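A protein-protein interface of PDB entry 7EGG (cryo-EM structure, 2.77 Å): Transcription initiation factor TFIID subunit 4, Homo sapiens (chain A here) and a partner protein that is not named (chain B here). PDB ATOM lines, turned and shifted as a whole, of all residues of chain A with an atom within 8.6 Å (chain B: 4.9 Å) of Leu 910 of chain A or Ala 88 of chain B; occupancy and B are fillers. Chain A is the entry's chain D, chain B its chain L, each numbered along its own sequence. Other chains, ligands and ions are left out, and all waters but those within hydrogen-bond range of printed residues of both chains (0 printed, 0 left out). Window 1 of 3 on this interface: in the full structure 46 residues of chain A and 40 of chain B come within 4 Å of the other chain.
OD1 of Asp 89 of chain B is in salt-bridge range of NH1 of Arg 881 of chain A (3.8 Å).
The side-chain hydroxyl of Thr 871 of chain A lies close to the backbone NH of Gln 907 of chain A. The side-chain hydroxyl of Ser 903 of chain A is in hydrogen-bond range of the backbone NH of Leu 873 of chain A. O of Val 902 of chain A sits at hydrogen-bond distance from OG1 of Thr 906 of chain A. The side-chain hydroxyl of Ser 918 of chain A lies within hydrogen-bond range of the backbone carbonyl oxygen of Val 914 of chain A.
Among the printed residues, pairs that only touch across the chains: Thr 871 of chain A with Leu 58 of chain B (3.8 Å), Thr 871 of chain A with Leu 66 of chain B (3.5 Å), Leu 873 of chain A with Ile 92 of chain B (3.5 Å), Leu 878 of chain A with Ile 92 of chain B (3.96 Å), Ala 905 of chain A with Phe 91 of chain B (3.2 Å), Thr 906 of chain A with Phe 91 of chain B (3.9 Å), Thr 906 of chain A with Ile 92 of chain B (3.6 Å), Arg 909 of chain A with Phe 91 of chain B (3.7 Å), Leu 910 of chain A with Leu 58 of chain B (3.8 Å), Leu 910 of chain A with Leu 63 of chain B (3.9 Å), Leu 910 of chain A with Leu 66 of chain B (3.8 Å), Leu 910 of chain A with Ala 88 of chain B (3.8 Å), Gln 911 of chain A with Leu 66 of chain B (3.4 Å), Leu 913 of chain A with Ile 87 of chain B (3.9 Å), Val 914 of chain A with Leu 66 of chain B (3.7 Å), Leu 1063 of chain A with Leu 84 of chain B (3.7 Å), Leu 1078 of chain A with Ile 87 of chain B (3.6 Å) and Leu 1078 of chain A with Asp 90 of chain B (3.2 Å).
Printed residues of chain B within 4 Å of Leu 878 of chain A: Ile 92. His 904 of chain A touches none of the printed residues of chain B. Of chain B, only Leu 58 (3.8 Å), Leu 63 (3.9 Å), Leu 66 (3.8 Å) and Ala 88 (3.8 Å) come within 4 Å of Leu 910 of chain A. Asn 912 of chain A touches none of the printed residues of chain B. Printed residues of chain A within 4 Å of Leu 84 of chain B: Leu 1063 (3.7 Å). Of chain A, only Leu 910 comes within 4 Å of Ala 88 of chain B.
Hydrophobic or aromatic side chains of chain B that line the printed part of chain A: Leu 58, Leu 63, Leu 66, Leu 84, Ile 87, Ala 88, Phe 91 and Ile 92. Of the 24 printed residues of chain A, 13 touch a printed residue of chain B. Among the printed residues, 19 pairs touch across the chains.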
ATOM      1  N   THR A 871      14.164   2.819 -21.697  1.00  0.00           N
ATOM      2  CA  THR A 871      15.308   2.252 -21.006  1.00  0.00           C
ATOM      3  C   THR A 871      16.381   1.833 -21.994  1.00  0.00           C
ATOM      4  O   THR A 871      17.550   2.154 -21.792  1.00  0.00           O
ATOM      5  CB  THR A 871      14.918   1.044 -20.150  1.00  0.00           C
ATOM      6  OG1 THR A 871      14.229   0.086 -20.961  1.00  0.00           O
ATOM      7  CG2 THR A 871      14.022   1.475 -19.012  1.00  0.00           C
ATOM      8  N   PHE A 872      15.963   1.123 -23.050  1.00  0.00           N
ATOM      9  CA  PHE A 872      16.835   0.625 -24.120  1.00  0.00           C
ATOM     10  C   PHE A 872      17.948  -0.256 -23.544  1.00  0.00           C
ATOM     11  O   PHE A 872      19.115   0.135 -23.464  1.00  0.00           O
ATOM     12  CB  PHE A 872      17.399   1.771 -24.974  1.00  0.00           C
ATOM     13  CG  PHE A 872      18.152   1.305 -26.189  1.00  0.00           C
ATOM     14  CD1 PHE A 872      17.510   0.578 -27.178  1.00  0.00           C
ATOM     15  CD2 PHE A 872      19.500   1.590 -26.338  1.00  0.00           C
ATOM     16  CE1 PHE A 872      18.197   0.144 -28.295  1.00  0.00           C
ATOM     17  CE2 PHE A 872      20.191   1.158 -27.453  1.00  0.00           C
ATOM     18  CZ  PHE A 872      19.539   0.435 -28.432  1.00  0.00           C
ATOM     19  N   LEU A 873      17.511  -1.420 -23.058  1.00  0.00           N
ATOM     20  CA  LEU A 873      18.371  -2.392 -22.387  1.00  0.00           C
ATOM     21  C   LEU A 873      19.557  -2.800 -23.256  1.00  0.00           C
ATOM     22  O   LEU A 873      19.480  -2.814 -24.489  1.00  0.00           O
ATOM     23  CB  LEU A 873      17.559  -3.635 -22.014  1.00  0.00           C
ATOM     24  CG  LEU A 873      16.957  -3.778 -20.612  1.00  0.00           C
ATOM     25  CD1 LEU A 873      16.156  -2.559 -20.198  1.00  0.00           C
ATOM     26  CD2 LEU A 873      16.088  -5.024 -20.547  1.00  0.00           C
ATOM     27  N   LEU A 878      21.612  -8.863 -22.216  1.00  0.00           N
ATOM     28  CA  LEU A 878      20.230  -9.324 -22.278  1.00  0.00           C
ATOM     29  C   LEU A 878      20.119 -10.616 -23.072  1.00  0.00           C
ATOM     30  O   LEU A 878      19.330 -11.498 -22.720  1.00  0.00           O
ATOM     31  CB  LEU A 878      19.335  -8.244 -22.882  1.00  0.00           C
ATOM     32  CG  LEU A 878      17.839  -8.535 -22.990  1.00  0.00           C
ATOM     33  CD1 LEU A 878      17.265  -8.956 -21.648  1.00  0.00           C
ATOM     34  CD2 LEU A 878      17.103  -7.325 -23.534  1.00  0.00           C
ATOM     35  N   ARG A 881      20.801 -13.350 -21.046  1.00  0.00           N
ATOM     36  CA  ARG A 881      19.790 -13.493 -20.005  1.00  0.00           C
ATOM     37  C   ARG A 881      18.578 -14.271 -20.508  1.00  0.00           C
ATOM     38  O   ARG A 881      18.019 -15.094 -19.773  1.00  0.00           O
ATOM     39  CB  ARG A 881      19.389 -12.110 -19.489  1.00  0.00           C
ATOM     40  CG  ARG A 881      18.204 -12.086 -18.549  1.00  0.00           C
ATOM     41  CD  ARG A 881      18.605 -12.506 -17.150  1.00  0.00           C
ATOM     42  NE  ARG A 881      17.682 -11.982 -16.148  1.00  0.00           N
ATOM     43  CZ  ARG A 881      17.793 -10.779 -15.596  1.00  0.00           C
ATOM     44  NH1 ARG A 881      16.908 -10.380 -14.695  1.00  0.00           N
ATOM     45  NH2 ARG A 881      18.791  -9.979 -15.942  1.00  0.00           N
ATOM     46  N   VAL A 902      12.167  -7.172 -26.505  1.00  0.00           N
ATOM     47  CA  VAL A 902      12.035  -7.219 -25.054  1.00  0.00           C
ATOM     48  C   VAL A 902      12.574  -5.929 -24.442  1.00  0.00           C
ATOM     49  O   VAL A 902      12.038  -5.428 -23.444  1.00  0.00           O
ATOM     50  CB  VAL A 902      12.745  -8.481 -24.522  1.00  0.00           C
ATOM     51  CG1 VAL A 902      12.838  -8.502 -23.004  1.00  0.00           C
ATOM     52  CG2 VAL A 902      12.032  -9.724 -25.018  1.00  0.00           C
ATOM     53  N   SER A 903      13.599  -5.340 -25.064  1.00  0.00           N
ATOM     54  CA  SER A 903      14.116  -4.055 -24.613  1.00  0.00           C
ATOM     55  C   SER A 903      13.126  -2.924 -24.863  1.00  0.00           C
ATOM     56  O   SER A 903      13.050  -1.985 -24.064  1.00  0.00           O
ATOM     57  CB  SER A 903      15.442  -3.758 -25.305  1.00  0.00           C
ATOM     58  OG  SER A 903      15.930  -2.487 -24.930  1.00  0.00           O
ATOM     59  N   HIS A 904      12.366  -2.988 -25.957  1.00  0.00           N
ATOM     60  CA  HIS A 904      11.280  -2.040 -26.160  1.00  0.00           C
ATOM     61  C   HIS A 904      10.083  -2.338 -25.271  1.00  0.00           C
ATOM     62  O   HIS A 904       9.294  -1.430 -24.990  1.00  0.00           O
ATOM     63  CB  HIS A 904      10.838  -2.040 -27.625  1.00  0.00           C
ATOM     64  CG  HIS A 904      11.711  -1.221 -28.521  1.00  0.00           C
ATOM     65  ND1 HIS A 904      11.297  -0.772 -29.755  1.00  0.00           N
ATOM     66  CD2 HIS A 904      12.977  -0.768 -28.361  1.00  0.00           C
ATOM     67  CE1 HIS A 904      12.270  -0.079 -30.319  1.00  0.00           C
ATOM     68  NE2 HIS A 904      13.301  -0.062 -29.493  1.00  0.00           N
ATOM     69  N   ALA A 905       9.933  -3.585 -24.827  1.00  0.00           N
ATOM     70  CA  ALA A 905       8.850  -3.943 -23.921  1.00  0.00           C
ATOM     71  C   ALA A 905       9.179  -3.593 -22.480  1.00  0.00           C
ATOM     72  O   ALA A 905       8.275  -3.289 -21.699  1.00  0.00           O
ATOM     73  CB  ALA A 905       8.553  -5.436 -24.031  1.00  0.00           C
ATOM     74  N   THR A 906      10.461  -3.638 -22.114  1.00  0.00           N
ATOM     75  CA  THR A 906      10.869  -3.231 -20.776  1.00  0.00           C
ATOM     76  C   THR A 906      10.824  -1.715 -20.637  1.00  0.00           C
ATOM     77  O   THR A 906      10.547  -1.196 -19.549  1.00  0.00           O
ATOM     78  CB  THR A 906      12.270  -3.774 -20.488  1.00  0.00           C
ATOM     79  OG1 THR A 906      12.291  -5.178 -20.767  1.00  0.00           O
ATOM     80  CG2 THR A 906      12.650  -3.591 -19.032  1.00  0.00           C
ATOM     81  N   GLN A 907      11.053  -0.996 -21.738  1.00  0.00           N
ATOM     82  CA  GLN A 907      10.991   0.460 -21.713  1.00  0.00           C
ATOM     83  C   GLN A 907       9.568   0.947 -21.489  1.00  0.00           C
ATOM     84  O   GLN A 907       9.324   1.795 -20.627  1.00  0.00           O
ATOM     85  CB  GLN A 907      11.555   1.029 -23.012  1.00  0.00           C
ATOM     86  CG  GLN A 907      11.193   2.480 -23.255  1.00  0.00           C
ATOM     87  CD  GLN A 907      11.904   3.058 -24.454  1.00  0.00           C
ATOM     88  OE1 GLN A 907      12.112   2.375 -25.456  1.00  0.00           O
ATOM     89  NE2 GLN A 907      12.284   4.325 -24.361  1.00  0.00           N
ATOM     90  N   GLN A 908       8.607   0.390 -22.227  1.00  0.00           N
ATOM     91  CA  GLN A 908       7.215   0.784 -22.052  1.00  0.00           C
ATOM     92  C   GLN A 908       6.601   0.249 -20.766  1.00  0.00           C
ATOM     93  O   GLN A 908       5.501   0.675 -20.406  1.00  0.00           O
ATOM     94  CB  GLN A 908       6.378   0.332 -23.249  1.00  0.00           C
ATOM     95  CG  GLN A 908       6.767   0.988 -24.563  1.00  0.00           C
ATOM     96  CD  GLN A 908       6.582   2.495 -24.545  1.00  0.00           C
ATOM     97  OE1 GLN A 908       7.457   3.244 -24.978  1.00  0.00           O
ATOM     98  NE2 GLN A 908       5.437   2.946 -24.048  1.00  0.00           N
ATOM     99  N   ARG A 909       7.272  -0.671 -20.073  1.00  0.00           N
ATOM    100  CA  ARG A 909       6.841  -1.050 -18.734  1.00  0.00           C
ATOM    101  C   ARG A 909       7.285  -0.021 -17.706  1.00  0.00           C
ATOM    102  O   ARG A 909       6.504   0.367 -16.833  1.00  0.00           O
ATOM    103  CB  ARG A 909       7.389  -2.431 -18.376  1.00  0.00           C
ATOM    104  CG  ARG A 909       7.225  -2.820 -16.918  1.00  0.00           C
ATOM    105  CD  ARG A 909       5.847  -3.390 -16.658  1.00  0.00           C
ATOM    106  NE  ARG A 909       5.641  -3.704 -15.250  1.00  0.00           N
ATOM    107  CZ  ARG A 909       4.961  -2.930 -14.411  1.00  0.00           C
ATOM    108  NH1 ARG A 909       4.815  -3.290 -13.144  1.00  0.00           N
ATOM    109  NH2 ARG A 909       4.429  -1.797 -14.842  1.00  0.00           N
ATOM    110  N   LEU A 910       8.527   0.450 -17.808  1.00  0.00           N
ATOM    111  CA  LEU A 910       9.033   1.394 -16.823  1.00  0.00           C
ATOM    112  C   LEU A 910       8.632   2.827 -17.137  1.00  0.00           C
ATOM    113  O   LEU A 910       8.472   3.628 -16.212  1.00  0.00           O
ATOM    114  CB  LEU A 910      10.553   1.282 -16.710  1.00  0.00           C
ATOM    115  CG  LEU A 910      11.103  -0.070 -16.246  1.00  0.00           C
ATOM    116  CD1 LEU A 910      12.567   0.058 -15.885  1.00  0.00           C
ATOM    117  CD2 LEU A 910      10.321  -0.630 -15.070  1.00  0.00           C
ATOM    118  N   GLN A 911       8.456   3.171 -18.416  1.00  0.00           N
ATOM    119  CA  GLN A 911       7.966   4.506 -18.747  1.00  0.00           C
ATOM    120  C   GLN A 911       6.502   4.668 -18.369  1.00  0.00           C
ATOM    121  O   GLN A 911       6.063   5.778 -18.053  1.00  0.00           O
ATOM    122  CB  GLN A 911       8.160   4.796 -20.231  1.00  0.00           C
ATOM    123  CG  GLN A 911       8.211   6.265 -20.568  1.00  0.00           C
ATOM    124  CD  GLN A 911       8.430   6.514 -22.039  1.00  0.00           C
ATOM    125  OE1 GLN A 911       7.480   6.580 -22.817  1.00  0.00           O
ATOM    126  NE2 GLN A 911       9.690   6.657 -22.435  1.00  0.00           N
ATOM    127  N   ASN A 912       5.736   3.578 -18.384  1.00  0.00           N
ATOM    128  CA  ASN A 912       4.388   3.608 -17.835  1.00  0.00           C
ATOM    129  C   ASN A 912       4.397   3.671 -16.315  1.00  0.00           C
ATOM    130  O   ASN A 912       3.376   4.018 -15.713  1.00  0.00           O
ATOM    131  CB  ASN A 912       3.601   2.384 -18.307  1.00  0.00           C
ATOM    132  CG  ASN A 912       2.105   2.546 -18.132  1.00  0.00           C
ATOM    133  OD1 ASN A 912       1.428   1.649 -17.630  1.00  0.00           O
ATOM    134  ND2 ASN A 912       1.580   3.695 -18.541  1.00  0.00           N
ATOM    135  N   LEU A 913       5.524   3.353 -15.682  1.00  0.00           N
ATOM    136  CA  LEU A 913       5.654   3.446 -14.236  1.00  0.00           C
ATOM    137  C   LEU A 913       6.406   4.689 -13.784  1.00  0.00           C
ATOM    138  O   LEU A 913       6.174   5.161 -12.669  1.00  0.00           O
ATOM    139  CB  LEU A 913       6.355   2.198 -13.691  1.00  0.00           C
ATOM    140  CG  LEU A 913       5.954   1.740 -12.291  1.00  0.00           C
ATOM    141  CD1 LEU A 913       4.461   1.491 -12.214  1.00  0.00           C
ATOM    142  CD2 LEU A 913       6.716   0.485 -11.930  1.00  0.00           C
ATOM    143  N   VAL A 914       7.294   5.234 -14.618  1.00  0.00           N
ATOM    144  CA  VAL A 914       7.951   6.496 -14.282  1.00  0.00           C
ATOM    145  C   VAL A 914       6.967   7.655 -14.415  1.00  0.00           C
ATOM    146  O   VAL A 914       6.925   8.553 -13.564  1.00  0.00           O
ATOM    147  CB  VAL A 914       9.209   6.684 -15.154  1.00  0.00           C
ATOM    148  CG1 VAL A 914       9.631   8.143 -15.256  1.00  0.00           C
ATOM    149  CG2 VAL A 914      10.357   5.853 -14.604  1.00  0.00           C
ATOM    150  N   GLU A 915       6.133   7.632 -15.462  1.00  0.00           N
ATOM    151  CA  GLU A 915       5.073   8.627 -15.607  1.00  0.00           C
ATOM    152  C   GLU A 915       4.025   8.509 -14.510  1.00  0.00           C
ATOM    153  O   GLU A 915       3.440   9.518 -14.105  1.00  0.00           O
ATOM    154  CB  GLU A 915       4.390   8.490 -16.966  1.00  0.00           C
ATOM    155  CG  GLU A 915       5.093   9.182 -18.115  1.00  0.00           C
ATOM    156  CD  GLU A 915       4.881   8.470 -19.434  1.00  0.00           C
ATOM    157  OE1 GLU A 915       3.777   7.927 -19.641  1.00  0.00           O
ATOM    158  OE2 GLU A 915       5.804   8.475 -20.272  1.00  0.00           O
ATOM    159  N   LYS A 916       3.781   7.296 -14.020  1.00  0.00           N
ATOM    160  CA  LYS A 916       2.777   7.099 -12.982  1.00  0.00           C
ATOM    161  C   LYS A 916       3.272   7.583 -11.624  1.00  0.00           C
ATOM    162  O   LYS A 916       2.492   8.126 -10.838  1.00  0.00           O
ATOM    163  CB  LYS A 916       2.379   5.628 -12.921  1.00  0.00           C
ATOM    164  CG  LYS A 916       0.980   5.375 -12.397  1.00  0.00           C
ATOM    165  CD  LYS A 916       0.607   3.911 -12.553  1.00  0.00           C
ATOM    166  CE  LYS A 916      -0.639   3.574 -11.754  1.00  0.00           C
ATOM    167  NZ  LYS A 916      -0.889   2.107 -11.719  1.00  0.00           N
ATOM    168  N   ILE A 917       4.560   7.406 -11.325  1.00  0.00           N
ATOM    169  CA  ILE A 917       5.074   7.899 -10.050  1.00  0.00           C
ATOM    170  C   ILE A 917       5.416   9.380 -10.107  1.00  0.00           C
ATOM    171  O   ILE A 917       5.577  10.002  -9.054  1.00  0.00           O
ATOM    172  CB  ILE A 917       6.307   7.119  -9.564  1.00  0.00           C
ATOM    173  CG1 ILE A 917       7.506   7.362 -10.482  1.00  0.00           C
ATOM    174  CG2 ILE A 917       5.994   5.637  -9.418  1.00  0.00           C
ATOM    175  CD1 ILE A 917       8.746   6.618 -10.068  1.00  0.00           C
ATOM    176  N   SER A 918       5.534   9.965 -11.301  1.00  0.00           N
ATOM    177  CA  SER A 918       5.775  11.398 -11.402  1.00  0.00           C
ATOM    178  C   SER A 918       4.519  12.218 -11.158  1.00  0.00           C
ATOM    179  O   SER A 918       4.616  13.342 -10.660  1.00  0.00           O
ATOM    180  CB  SER A 918       6.352  11.746 -12.773  1.00  0.00           C
ATOM    181  OG  SER A 918       7.720  11.398 -12.849  1.00  0.00           O
ATOM    182  N   LEU A1063       6.557   5.235  -5.189  1.00  0.00           N
ATOM    183  CA  LEU A1063       6.649   3.996  -5.947  1.00  0.00           C
ATOM    184  C   LEU A1063       5.727   2.929  -5.372  1.00  0.00           C
ATOM    185  O   LEU A1063       5.122   2.164  -6.127  1.00  0.00           O
ATOM    186  CB  LEU A1063       8.094   3.506  -5.971  1.00  0.00           C
ATOM    187  CG  LEU A1063       8.407   2.321  -6.882  1.00  0.00           C
ATOM    188  CD1 LEU A1063       9.630   2.620  -7.703  1.00  0.00           C
ATOM    189  CD2 LEU A1063       8.634   1.075  -6.062  1.00  0.00           C
ATOM    190  N   LEU A1078       7.539  -8.284  -4.213  1.00  0.00           N
ATOM    191  CA  LEU A1078       8.368  -7.105  -4.397  1.00  0.00           C
ATOM    192  C   LEU A1078       7.756  -5.877  -3.739  1.00  0.00           C
ATOM    193  O   LEU A1078       8.491  -4.983  -3.308  1.00  0.00           O
ATOM    194  CB  LEU A1078       8.601  -6.866  -5.894  1.00  0.00           C
ATOM    195  CG  LEU A1078       9.778  -6.004  -6.370  1.00  0.00           C
ATOM    196  CD1 LEU A1078      10.255  -6.518  -7.715  1.00  0.00           C
ATOM    197  CD2 LEU A1078       9.436  -4.534  -6.478  1.00  0.00           C
ATOM    198  N   LEU B  58      20.156  -3.174 -17.193  1.00  0.00           N
ATOM    199  CA  LEU B  58      19.786  -1.765 -17.168  1.00  0.00           C
ATOM    200  C   LEU B  58      20.858  -1.001 -16.404  1.00  0.00           C
ATOM    201  O   LEU B  58      21.120  -1.293 -15.232  1.00  0.00           O
ATOM    202  CB  LEU B  58      18.403  -1.566 -16.542  1.00  0.00           C
ATOM    203  CG  LEU B  58      17.807  -0.162 -16.567  1.00  0.00           C
ATOM    204  CD1 LEU B  58      17.934   0.464 -17.946  1.00  0.00           C
ATOM    205  CD2 LEU B  58      16.349  -0.233 -16.158  1.00  0.00           C
ATOM    206  N   LEU B  63      18.138   4.759 -17.238  1.00  0.00           N
ATOM    207  CA  LEU B  63      16.931   4.932 -16.440  1.00  0.00           C
ATOM    208  C   LEU B  63      16.745   6.389 -16.042  1.00  0.00           C
ATOM    209  O   LEU B  63      15.612   6.877 -15.958  1.00  0.00           O
ATOM    210  CB  LEU B  63      16.990   4.039 -15.202  1.00  0.00           C
ATOM    211  CG  LEU B  63      15.731   3.965 -14.341  1.00  0.00           C
ATOM    212  CD1 LEU B  63      14.620   3.234 -15.068  1.00  0.00           C
ATOM    213  CD2 LEU B  63      16.045   3.295 -13.030  1.00  0.00           C
ATOM    214  N   LEU B  66      15.176   8.081 -18.816  1.00  0.00           N
ATOM    215  CA  LEU B  66      13.744   7.822 -18.867  1.00  0.00           C
ATOM    216  C   LEU B  66      12.965   8.766 -17.966  1.00  0.00           C
ATOM    217  O   LEU B  66      11.771   8.979 -18.193  1.00  0.00           O
ATOM    218  CB  LEU B  66      13.454   6.376 -18.476  1.00  0.00           C
ATOM    219  CG  LEU B  66      12.173   5.768 -19.048  1.00  0.00           C
ATOM    220  CD1 LEU B  66      12.323   5.530 -20.537  1.00  0.00           C
ATOM    221  CD2 LEU B  66      11.826   4.481 -18.331  1.00  0.00           C
ATOM    222  N   LEU B  84      13.175   0.079  -8.989  1.00  0.00           N
ATOM    223  CA  LEU B  84      12.793   0.143 -10.416  1.00  0.00           C
ATOM    224  C   LEU B  84      13.633  -0.863 -11.191  1.00  0.00           C
ATOM    225  O   LEU B  84      13.062  -1.580 -12.017  1.00  0.00           O
ATOM    226  CB  LEU B  84      12.975   1.576 -10.915  1.00  0.00           C
ATOM    227  CG  LEU B  84      11.784   2.498 -10.699  1.00  0.00           C
ATOM    228  CD1 LEU B  84      12.179   3.942 -10.936  1.00  0.00           C
ATOM    229  CD2 LEU B  84      10.632   2.108 -11.605  1.00  0.00           C
ATOM    230  N   LEU B  85      14.917  -0.970 -10.881  1.00  0.00           N
ATOM    231  CA  LEU B  85      15.777  -1.970 -11.550  1.00  0.00           C
ATOM    232  C   LEU B  85      15.293  -3.379 -11.221  1.00  0.00           C
ATOM    233  O   LEU B  85      15.193  -4.189 -12.137  1.00  0.00           O
ATOM    234  CB  LEU B  85      17.230  -1.741 -11.141  1.00  0.00           C
ATOM    235  CG  LEU B  85      17.844  -0.401 -11.528  1.00  0.00           C
ATOM    236  CD1 LEU B  85      19.356  -0.478 -11.491  1.00  0.00           C
ATOM    237  CD2 LEU B  85      17.391   0.004 -12.905  1.00  0.00           C
ATOM    238  N   GLN B  86      14.909  -3.640  -9.983  1.00  0.00           N
ATOM    239  CA  GLN B  86      14.357  -4.974  -9.641  1.00  0.00           C
ATOM    240  C   GLN B  86      13.070  -5.246 -10.395  1.00  0.00           C
ATOM    241  O   GLN B  86      12.915  -6.361 -10.841  1.00  0.00           O
ATOM    242  CB  GLN B  86      13.966  -5.091  -8.176  1.00  0.00           C
ATOM    243  CG  GLN B  86      15.109  -4.857  -7.203  1.00  0.00           C
ATOM    244  CD  GLN B  86      14.624  -4.919  -5.777  1.00  0.00           C
ATOM    245  OE1 GLN B  86      13.771  -5.735  -5.430  1.00  0.00           O
ATOM    246  NE2 GLN B  86      15.164  -4.051  -4.936  1.00  0.00           N
ATOM    247  N   ILE B  87      12.193  -4.263 -10.522  1.00  0.00           N
ATOM    248  CA  ILE B  87      10.913  -4.425 -11.261  1.00  0.00           C
ATOM    249  C   ILE B  87      11.244  -4.746 -12.712  1.00  0.00           C
ATOM    250  O   ILE B  87      10.671  -5.683 -13.221  1.00  0.00           O
ATOM    251  CB  ILE B  87      10.004  -3.187 -11.129  1.00  0.00           C
ATOM    252  CG1 ILE B  87       9.577  -2.931  -9.685  1.00  0.00           C
ATOM    253  CG2 ILE B  87       8.801  -3.297 -12.048  1.00  0.00           C
ATOM    254  CD1 ILE B  87       8.964  -1.574  -9.464  1.00  0.00           C
ATOM    255  N   ALA B  88      12.222  -4.074 -13.297  1.00  0.00           N
ATOM    256  CA  ALA B  88      12.611  -4.358 -14.688  1.00  0.00           C
ATOM    257  C   ALA B  88      13.107  -5.785 -14.788  1.00  0.00           C
ATOM    258  O   ALA B  88      12.706  -6.476 -15.713  1.00  0.00           O
ATOM    259  CB  ALA B  88      13.729  -3.451 -15.066  1.00  0.00           C
ATOM    260  N   ASP B  89      13.939  -6.213 -13.852  1.00  0.00           N
ATOM    261  CA  ASP B  89      14.529  -7.559 -13.952  1.00  0.00           C
ATOM    262  C   ASP B  89      13.402  -8.574 -13.848  1.00  0.00           C
ATOM    263  O   ASP B  89      13.368  -9.536 -14.634  1.00  0.00           O
ATOM    264  CB  ASP B  89      15.614  -7.695 -12.898  1.00  0.00           C
ATOM    265  CG  ASP B  89      16.944  -7.113 -13.327  1.00  0.00           C
ATOM    266  OD1 ASP B  89      17.022  -6.613 -14.461  1.00  0.00           O
ATOM    267  OD2 ASP B  89      17.889  -7.176 -12.523  1.00  0.00           O
ATOM    268  N   ASP B  90      12.477  -8.326 -12.947  1.00  0.00           N
ATOM    269  CA  ASP B  90      11.378  -9.281 -12.732  1.00  0.00           C
ATOM    270  C   ASP B  90      10.517  -9.334 -13.984  1.00  0.00           C
ATOM    271  O   ASP B  90      10.095 -10.435 -14.350  1.00  0.00           O
ATOM    272  CB  ASP B  90      10.581  -8.874 -11.510  1.00  0.00           C
ATOM    273  CG  ASP B  90      11.293  -9.171 -10.205  1.00  0.00           C
ATOM    274  OD1 ASP B  90      12.537  -9.231 -10.219  1.00  0.00           O
ATOM    275  OD2 ASP B  90      10.596  -9.351  -9.185  1.00  0.00           O
ATOM    276  N   PHE B  91      10.276  -8.192 -14.619  1.00  0.00           N
ATOM    277  CA  PHE B  91       9.445  -8.145 -15.835  1.00  0.00           C
ATOM    278  C   PHE B  91      10.146  -8.973 -16.878  1.00  0.00           C
ATOM    279  O   PHE B  91       9.519  -9.871 -17.416  1.00  0.00           O
ATOM    280  CB  PHE B  91       9.407  -6.731 -16.398  1.00  0.00           C
ATOM    281  CG  PHE B  91       8.494  -6.528 -17.576  1.00  0.00           C
ATOM    282  CD1 PHE B  91       7.140  -6.790 -17.473  1.00  0.00           C
ATOM    283  CD2 PHE B  91       8.990  -6.059 -18.777  1.00  0.00           C
ATOM    284  CE1 PHE B  91       6.302  -6.595 -18.555  1.00  0.00           C
ATOM    285  CE2 PHE B  91       8.148  -5.865 -19.858  1.00  0.00           C
ATOM    286  CZ  PHE B  91       6.807  -6.132 -19.743  1.00  0.00           C
ATOM    287  N   ILE B  92      11.441  -8.763 -17.047  1.00  0.00           N
ATOM    288  CA  ILE B  92      12.106  -9.507 -18.140  1.00  0.00           C
ATOM    289  C   ILE B  92      11.917 -10.981 -17.819  1.00  0.00           C
ATOM    290  O   ILE B  92      11.358 -11.684 -18.661  1.00  0.00           O
ATOM    291  CB  ILE B  92      13.588  -9.130 -18.234  1.00  0.00           C
ATOM    292  CG1 ILE B  92      13.776  -7.648 -18.545  1.00  0.00           C
ATOM    293  CG2 ILE B  92      14.305 -10.012 -19.238  1.00  0.00           C
ATOM    294  CD1 ILE B  92      15.029  -7.081 -17.941  1.00  0.00           C
